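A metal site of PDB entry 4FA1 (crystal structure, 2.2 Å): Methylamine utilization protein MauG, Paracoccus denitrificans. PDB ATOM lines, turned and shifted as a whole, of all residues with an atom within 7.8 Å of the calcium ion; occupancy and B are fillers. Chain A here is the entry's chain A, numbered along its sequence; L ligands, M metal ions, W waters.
The backbone NH (N) of Met 279 is in hydrogen-bond range of an oxygen (O1) of the ligand. N of His 280 sits at hydrogen-bond distance from O3 of the ligand (2.7 Å). An oxygen (O4) of the ligand is in hydrogen-bond range of a ring nitrogen (ND1) of His 280.
O of Asn 66 lies within hydrogen-bond range of NE1 of Trp 93 (2.9 Å). The backbone carbonyl oxygen (O) of Leu 51 is in hydrogen-bond range of the side-chain amide nitrogen (ND2) of Asn 66, at 3.4 Å. O of Ala 52 is in hydrogen-bond range of ND2 of Asn 66 (3.0 Å). O of His 280 lies within hydrogen-bond range of N of Asn 66 (2.7 Å).
Within 4 Å of the calcium ion: Asn 66, Thr 275 and Pro 277. Along chain A the residues within 4 Å of the calcium ion span positions 66 to 277.
The calcium ion is bound by OD1 of Asn 66 (2.1 Å), water W3 (2.3 Å), O of Thr 275 (2.3 Å), O of Pro 277 (2.4 Å), water W1 (2.4 Å), water W2 (2.5 Å) and water W4 (2.6 Å). The calcium ion has seven donor atoms within binding distance.
Water W3 lies within hydrogen-bond range of the side-chain hydroxyl (OG1) of Thr 275 (2.5 Å) and an oxygen (O2) of the ligand (3.1 Å). Water W4 bridges O of Gly 276 and ND2 of Asn 66. Water W2 lies within hydrogen-bond range of an oxygen (O1) of the ligand (2.9 Å) and the backbone carbonyl oxygen of Met 279 (3.1 Å).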
ATOM      1  N   ARG A  39      15.518 -25.837   7.781  1.00  0.00           N
ATOM      2  CA  ARG A  39      15.155 -25.540   6.393  1.00  0.00           C
ATOM      3  C   ARG A  39      15.330 -26.726   5.465  1.00  0.00           C
ATOM      4  O   ARG A  39      15.944 -26.606   4.384  1.00  0.00           O
ATOM      5  CB  ARG A  39      15.899 -24.312   5.864  1.00  0.00           C
ATOM      6  CG  ARG A  39      15.360 -23.828   4.525  1.00  0.00           C
ATOM      7  CD  ARG A  39      15.964 -22.494   4.095  1.00  0.00           C
ATOM      8  NE  ARG A  39      15.691 -22.200   2.686  1.00  0.00           N
ATOM      9  CZ  ARG A  39      14.857 -21.272   2.258  1.00  0.00           C
ATOM     10  NH1 ARG A  39      14.189 -20.511   3.121  1.00  0.00           N
ATOM     11  NH2 ARG A  39      14.679 -21.085   0.947  1.00  0.00           N
ATOM     12  N   THR A  42      18.905 -27.290   4.331  1.00  0.00           N
ATOM     13  CA  THR A  42      19.520 -26.371   3.387  1.00  0.00           C
ATOM     14  C   THR A  42      19.824 -25.066   4.128  1.00  0.00           C
ATOM     15  O   THR A  42      19.418 -24.858   5.294  1.00  0.00           O
ATOM     16  CB  THR A  42      18.615 -26.058   2.147  1.00  0.00           C
ATOM     17  OG1 THR A  42      17.383 -25.402   2.540  1.00  0.00           O
ATOM     18  CG2 THR A  42      18.312 -27.309   1.387  1.00  0.00           C
ATOM     19  N   ASP A  43      20.491 -24.184   3.374  1.00  0.00           N
ATOM     20  CA  ASP A  43      21.101 -22.981   3.903  1.00  0.00           C
ATOM     21  C   ASP A  43      20.184 -21.775   3.766  1.00  0.00           C
ATOM     22  O   ASP A  43      19.944 -21.317   2.633  1.00  0.00           O
ATOM     23  CB  ASP A  43      22.405 -22.688   3.152  1.00  0.00           C
ATOM     24  CG  ASP A  43      23.337 -21.700   3.916  1.00  0.00           C
ATOM     25  OD1 ASP A  43      24.494 -21.540   3.470  1.00  0.00           O
ATOM     26  OD2 ASP A  43      22.900 -21.089   4.941  1.00  0.00           O
ATOM     27  N   LEU A  51      20.558 -16.591  -1.964  1.00  0.00           N
ATOM     28  CA  LEU A  51      20.548 -17.911  -1.342  1.00  0.00           C
ATOM     29  C   LEU A  51      20.999 -18.990  -2.320  1.00  0.00           C
ATOM     30  O   LEU A  51      20.821 -20.199  -2.060  1.00  0.00           O
ATOM     31  CB  LEU A  51      19.143 -18.199  -0.823  1.00  0.00           C
ATOM     32  CG  LEU A  51      18.817 -18.038   0.662  1.00  0.00           C
ATOM     33  CD1 LEU A  51      19.342 -16.755   1.242  1.00  0.00           C
ATOM     34  CD2 LEU A  51      17.287 -18.124   0.866  1.00  0.00           C
ATOM     35  N   ALA A  52      21.620 -18.543  -3.416  1.00  0.00           N
ATOM     36  CA  ALA A  52      21.967 -19.428  -4.532  1.00  0.00           C
ATOM     37  C   ALA A  52      23.118 -20.332  -4.156  1.00  0.00           C
ATOM     38  O   ALA A  52      23.106 -21.516  -4.504  1.00  0.00           O
ATOM     39  CB  ALA A  52      22.307 -18.627  -5.801  1.00  0.00           C
ATOM     40  N   ASN A  66      24.405 -24.726  -5.409  1.00  0.00           N
ATOM     41  CA  ASN A  66      23.368 -24.631  -4.399  1.00  0.00           C
ATOM     42  C   ASN A  66      23.451 -25.767  -3.396  1.00  0.00           C
ATOM     43  O   ASN A  66      23.662 -26.925  -3.785  1.00  0.00           O
ATOM     44  CB  ASN A  66      22.012 -24.662  -5.056  1.00  0.00           C
ATOM     45  CG  ASN A  66      20.916 -24.377  -4.094  1.00  0.00           C
ATOM     46  OD1 ASN A  66      19.909 -25.093  -4.033  1.00  0.00           O
ATOM     47  ND2 ASN A  66      21.125 -23.347  -3.281  1.00  0.00           N
ATOM     48  N   THR A  67      23.265 -25.429  -2.123  1.00  0.00           N
ATOM     49  CA  THR A  67      23.330 -26.432  -1.068  1.00  0.00           C
ATOM     50  C   THR A  67      22.071 -27.312  -1.152  1.00  0.00           C
ATOM     51  O   THR A  67      20.979 -26.834  -0.988  1.00  0.00           O
ATOM     52  CB  THR A  67      23.540 -25.750   0.306  1.00  0.00           C
ATOM     53  OG1 THR A  67      24.864 -25.211   0.359  1.00  0.00           O
ATOM     54  CG2 THR A  67      23.316 -26.717   1.491  1.00  0.00           C
ATOM     55  N   PRO A  68      22.227 -28.615  -1.448  1.00  0.00           N
ATOM     56  CA  PRO A  68      21.051 -29.490  -1.466  1.00  0.00           C
ATOM     57  C   PRO A  68      20.558 -30.007  -0.074  1.00  0.00           C
ATOM     58  O   PRO A  68      21.318 -30.068   0.926  1.00  0.00           O
ATOM     59  CB  PRO A  68      21.504 -30.659  -2.336  1.00  0.00           C
ATOM     60  CG  PRO A  68      22.966 -30.711  -2.133  1.00  0.00           C
ATOM     61  CD  PRO A  68      23.453 -29.341  -1.743  1.00  0.00           C
ATOM     62  N   THR A  69      19.299 -30.383  -0.024  1.00  0.00           N
ATOM     63  CA  THR A  69      18.748 -31.041   1.140  1.00  0.00           C
ATOM     64  C   THR A  69      19.480 -32.370   1.402  1.00  0.00           C
ATOM     65  O   THR A  69      19.973 -33.027   0.471  1.00  0.00           O
ATOM     66  CB  THR A  69      17.259 -31.355   0.933  1.00  0.00           C
ATOM     67  OG1 THR A  69      16.747 -31.934   2.114  1.00  0.00           O
ATOM     68  CG2 THR A  69      17.068 -32.371  -0.231  1.00  0.00           C
ATOM     69  N   TRP A  93      25.891 -32.893  -6.658  1.00  0.00           N
ATOM     70  CA  TRP A  93      25.193 -32.634  -7.910  1.00  0.00           C
ATOM     71  C   TRP A  93      25.854 -33.273  -9.129  1.00  0.00           C
ATOM     72  O   TRP A  93      25.207 -33.410 -10.186  1.00  0.00           O
ATOM     73  CB  TRP A  93      25.124 -31.150  -8.141  1.00  0.00           C
ATOM     74  CG  TRP A  93      24.139 -30.380  -7.285  1.00  0.00           C
ATOM     75  CD1 TRP A  93      24.428 -29.621  -6.196  1.00  0.00           C
ATOM     76  CD2 TRP A  93      22.729 -30.236  -7.508  1.00  0.00           C
ATOM     77  NE1 TRP A  93      23.281 -29.028  -5.707  1.00  0.00           N
ATOM     78  CE2 TRP A  93      22.231 -29.374  -6.516  1.00  0.00           C
ATOM     79  CE3 TRP A  93      21.838 -30.755  -8.468  1.00  0.00           C
ATOM     80  CZ2 TRP A  93      20.855 -29.029  -6.425  1.00  0.00           C
ATOM     81  CZ3 TRP A  93      20.469 -30.405  -8.381  1.00  0.00           C
ATOM     82  CH2 TRP A  93      19.999 -29.536  -7.378  1.00  0.00           C
ATOM     83  N   VAL A 272      10.853 -30.199  -2.196  1.00  0.00           N
ATOM     84  CA  VAL A 272      11.251 -29.200  -3.191  1.00  0.00           C
ATOM     85  C   VAL A 272      10.585 -27.845  -2.913  1.00  0.00           C
ATOM     86  O   VAL A 272      11.152 -26.791  -3.184  1.00  0.00           O
ATOM     87  CB  VAL A 272      11.086 -29.657  -4.654  1.00  0.00           C
ATOM     88  CG1 VAL A 272       9.591 -29.818  -5.073  1.00  0.00           C
ATOM     89  CG2 VAL A 272      11.822 -28.723  -5.579  1.00  0.00           C
ATOM     90  N   VAL A 274      10.301 -26.204  -0.305  1.00  0.00           N
ATOM     91  CA  VAL A 274      10.922 -25.438   0.761  1.00  0.00           C
ATOM     92  C   VAL A 274      12.453 -25.406   0.670  1.00  0.00           C
ATOM     93  O   VAL A 274      13.137 -25.052   1.663  1.00  0.00           O
ATOM     94  CB  VAL A 274      10.480 -25.972   2.200  1.00  0.00           C
ATOM     95  CG1 VAL A 274       8.960 -25.895   2.390  1.00  0.00           C
ATOM     96  CG2 VAL A 274      10.941 -27.403   2.413  1.00  0.00           C
ATOM     97  N   THR A 275      13.021 -25.809  -0.473  1.00  0.00           N
ATOM     98  CA  THR A 275      14.466 -25.681  -0.631  1.00  0.00           C
ATOM     99  C   THR A 275      14.956 -24.827  -1.810  1.00  0.00           C
ATOM    100  O   THR A 275      16.008 -25.095  -2.331  1.00  0.00           O
ATOM    101  CB  THR A 275      15.124 -27.022  -0.694  1.00  0.00           C
ATOM    102  OG1 THR A 275      14.692 -27.700  -1.882  1.00  0.00           O
ATOM    103  CG2 THR A 275      14.764 -27.804   0.504  1.00  0.00           C
ATOM    104  N   GLY A 276      14.201 -23.814  -2.214  1.00  0.00           N
ATOM    105  CA  GLY A 276      14.690 -22.845  -3.216  1.00  0.00           C
ATOM    106  C   GLY A 276      15.903 -22.107  -2.658  1.00  0.00           C
ATOM    107  O   GLY A 276      16.127 -22.146  -1.426  1.00  0.00           O
ATOM    108  N   PRO A 277      16.683 -21.437  -3.551  1.00  0.00           N
ATOM    109  CA  PRO A 277      16.484 -21.451  -4.999  1.00  0.00           C
ATOM    110  C   PRO A 277      16.844 -22.807  -5.692  1.00  0.00           C
ATOM    111  O   PRO A 277      17.361 -23.746  -5.042  1.00  0.00           O
ATOM    112  CB  PRO A 277      17.366 -20.289  -5.472  1.00  0.00           C
ATOM    113  CG  PRO A 277      18.419 -20.279  -4.521  1.00  0.00           C
ATOM    114  CD  PRO A 277      17.811 -20.570  -3.205  1.00  0.00           C
ATOM    115  N   TYR A 278      16.532 -22.933  -6.965  1.00  0.00           N
ATOM    116  CA  TYR A 278      16.517 -24.244  -7.606  1.00  0.00           C
ATOM    117  C   TYR A 278      17.693 -24.483  -8.550  1.00  0.00           C
ATOM    118  O   TYR A 278      18.413 -23.554  -8.900  1.00  0.00           O
ATOM    119  CB  TYR A 278      15.145 -24.535  -8.233  1.00  0.00           C
ATOM    120  CG  TYR A 278      14.089 -24.461  -7.181  1.00  0.00           C
ATOM    121  CD1 TYR A 278      13.265 -23.348  -7.050  1.00  0.00           C
ATOM    122  CD2 TYR A 278      13.972 -25.462  -6.243  1.00  0.00           C
ATOM    123  CE1 TYR A 278      12.326 -23.280  -6.028  1.00  0.00           C
ATOM    124  CE2 TYR A 278      13.039 -25.399  -5.245  1.00  0.00           C
ATOM    125  CZ  TYR A 278      12.213 -24.335  -5.149  1.00  0.00           C
ATOM    126  OH  TYR A 278      11.298 -24.299  -4.131  1.00  0.00           O
ATOM    127  N   MET A 279      17.903 -25.762  -8.804  1.00  0.00           N
ATOM    128  CA  MET A 279      18.874 -26.288  -9.753  1.00  0.00           C
ATOM    129  C   MET A 279      20.236 -26.224  -9.112  1.00  0.00           C
ATOM    130  O   MET A 279      20.411 -25.682  -8.007  1.00  0.00           O
ATOM    131  CB  MET A 279      18.827 -25.571 -11.107  1.00  0.00           C
ATOM    132  CG  MET A 279      17.420 -25.568 -11.751  1.00  0.00           C
ATOM    133  SD  MET A 279      16.811 -27.231 -12.100  1.00  0.00           S
ATOM    134  CE  MET A 279      15.115 -26.971 -12.632  1.00  0.00           C
ATOM    135  N   HIS A 280      21.195 -26.820  -9.801  1.00  0.00           N
ATOM    136  CA  HIS A 280      22.485 -27.043  -9.236  1.00  0.00           C
ATOM    137  C   HIS A 280      23.146 -25.720  -8.827  1.00  0.00           C
ATOM    138  O   HIS A 280      23.976 -25.696  -7.939  1.00  0.00           O
ATOM    139  CB  HIS A 280      23.327 -27.857 -10.207  1.00  0.00           C
ATOM    140  CG  HIS A 280      23.652 -27.119 -11.472  1.00  0.00           C
ATOM    141  ND1 HIS A 280      23.024 -27.374 -12.669  1.00  0.00           N
ATOM    142  CD2 HIS A 280      24.555 -26.138 -11.724  1.00  0.00           C
ATOM    143  CE1 HIS A 280      23.520 -26.574 -13.608  1.00  0.00           C
ATOM    144  NE2 HIS A 280      24.441 -25.808 -13.056  1.00  0.00           N
ATOM    145  N   ASN A 281      22.744 -24.629  -9.464  1.00  0.00           N
ATOM    146  CA  ASN A 281      23.359 -23.323  -9.272  1.00  0.00           C
ATOM    147  C   ASN A 281      22.455 -22.300  -8.586  1.00  0.00           C
ATOM    148  O   ASN A 281      22.760 -21.144  -8.585  1.00  0.00           O
ATOM    149  CB  ASN A 281      23.896 -22.738 -10.625  1.00  0.00           C
ATOM    150  CG  ASN A 281      22.788 -22.572 -11.676  1.00  0.00           C
ATOM    151  OD1 ASN A 281      21.604 -22.608 -11.356  1.00  0.00           O
ATOM    152  ND2 ASN A 281      23.182 -22.366 -12.947  1.00  0.00           N
ATOM    153  N   GLY A 282      21.326 -22.733  -8.039  1.00  0.00           N
ATOM    154  CA  GLY A 282      20.379 -21.781  -7.456  1.00  0.00           C
ATOM    155  C   GLY A 282      19.738 -20.757  -8.395  1.00  0.00           C
ATOM    156  O   GLY A 282      19.066 -19.843  -7.915  1.00  0.00           O
ATOM    157  N   PHE A 284      17.182 -20.222 -10.199  1.00  0.00           N
ATOM    158  CA  PHE A 284      15.760 -19.908 -10.142  1.00  0.00           C
ATOM    159  C   PHE A 284      15.377 -19.813  -8.691  1.00  0.00           C
ATOM    160  O   PHE A 284      15.543 -20.770  -7.956  1.00  0.00           O
ATOM    161  CB  PHE A 284      14.951 -21.028 -10.825  1.00  0.00           C
ATOM    162  CG  PHE A 284      15.353 -21.282 -12.229  1.00  0.00           C
ATOM    163  CD1 PHE A 284      15.740 -20.226 -13.056  1.00  0.00           C
ATOM    164  CD2 PHE A 284      15.345 -22.566 -12.747  1.00  0.00           C
ATOM    165  CE1 PHE A 284      16.113 -20.439 -14.359  1.00  0.00           C
ATOM    166  CE2 PHE A 284      15.721 -22.799 -14.080  1.00  0.00           C
ATOM    167  CZ  PHE A 284      16.101 -21.739 -14.884  1.00  0.00           C
HETATM  168 FE1  LIG L   1      13.291 -31.939 -13.511  1.00  0.00          FE
HETATM  169  C1  LIG L   1      15.569 -30.288 -11.476  1.00  0.00           C
HETATM  170  C2  LIG L   1      10.750 -30.588 -11.814  1.00  0.00           C
HETATM  171  C3  LIG L   1      11.155 -32.940 -16.027  1.00  0.00           C
HETATM  172  C4  LIG L   1      15.727 -33.910 -14.743  1.00  0.00           C
HETATM  173  N1  LIG L   1      13.168 -30.631 -11.900  1.00  0.00           N
HETATM  174  C5  LIG L   1      14.157 -30.048 -11.208  1.00  0.00           C
HETATM  175  C6  LIG L   1      13.705 -29.149 -10.142  1.00  0.00           C
HETATM  176  C7  LIG L   1      12.316 -29.222 -10.236  1.00  0.00           C
HETATM  177  C8  LIG L   1      12.072 -30.143 -11.372  1.00  0.00           C
HETATM  178  C9  LIG L   1      11.276 -28.527  -9.425  1.00  0.00           C
HETATM  179  C10 LIG L   1      14.597 -28.385  -9.183  1.00  0.00           C
HETATM  180  C11 LIG L   1      14.693 -29.222  -7.883  1.00  0.00           C
HETATM  181  C12 LIG L   1      15.890 -28.952  -6.988  1.00  0.00           C
HETATM  182  O1  LIG L   1      16.729 -28.134  -7.430  1.00  0.00           O
HETATM  183  O2  LIG L   1      16.056 -29.547  -5.842  1.00  0.00           O
HETATM  184  N2  LIG L   1      11.279 -31.811 -13.860  1.00  0.00           N
HETATM  185  C13 LIG L   1      10.386 -31.257 -13.049  1.00  0.00           C
HETATM  186  C14 LIG L   1       9.001 -31.337 -13.529  1.00  0.00           C
HETATM  187  C15 LIG L   1       9.117 -32.018 -14.741  1.00  0.00           C
HETATM  188  C16 LIG L   1      10.553 -32.286 -14.863  1.00  0.00           C
HETATM  189  C17 LIG L   1       7.820 -30.796 -12.764  1.00  0.00           C
HETATM  190  C18 LIG L   1       8.077 -32.405 -15.751  1.00  0.00           C
HETATM  191  C19 LIG L   1       7.525 -31.120 -16.329  1.00  0.00           C
HETATM  192  N3  LIG L   1      13.427 -33.226 -15.118  1.00  0.00           N
HETATM  193  C20 LIG L   1      12.498 -33.526 -16.031  1.00  0.00           C
HETATM  194  C21 LIG L   1      12.943 -34.476 -17.055  1.00  0.00           C
HETATM  195  C22 LIG L   1      14.247 -34.772 -16.710  1.00  0.00           C
HETATM  196  C23 LIG L   1      14.476 -33.950 -15.490  1.00  0.00           C
HETATM  197  C24 LIG L   1      12.108 -34.988 -18.208  1.00  0.00           C
HETATM  198  C25 LIG L   1      15.217 -35.716 -17.409  1.00  0.00           C
HETATM  199  C26 LIG L   1      15.320 -35.423 -18.909  1.00  0.00           C
HETATM  200  N4  LIG L   1      15.322 -32.094 -13.144  1.00  0.00           N
HETATM  201  C27 LIG L   1      16.182 -32.886 -13.803  1.00  0.00           C
HETATM  202  C28 LIG L   1      17.595 -32.705 -13.433  1.00  0.00           C
HETATM  203  C29 LIG L   1      17.542 -31.680 -12.504  1.00  0.00           C
HETATM  204  C30 LIG L   1      16.104 -31.352 -12.368  1.00  0.00           C
HETATM  205  C31 LIG L   1      18.786 -33.448 -13.981  1.00  0.00           C
HETATM  206  C32 LIG L   1      18.694 -30.978 -11.844  1.00  0.00           C
HETATM  207  C33 LIG L   1      19.060 -30.021 -12.982  1.00  0.00           C
HETATM  208  C34 LIG L   1      20.344 -29.271 -12.750  1.00  0.00           C
HETATM  209  O3  LIG L   1      20.457 -28.551 -11.722  1.00  0.00           O
HETATM  210  O4  LIG L   1      21.242 -29.381 -13.612  1.00  0.00           O
HETATM  211 CA    CA M   1      17.857 -25.587  -3.630  1.00  0.00          CA
HETATM  212  O   HOH W   1      18.362 -27.185  -1.912  1.00  0.00           O
HETATM  213  O   HOH W   2      18.553 -26.668  -5.776  1.00  0.00           O
HETATM  214  O   HOH W   3      16.190 -27.161  -3.849  1.00  0.00           O
HETATM  215  O   HOH W   4      18.287 -23.669  -1.936  1.00  0.00           O
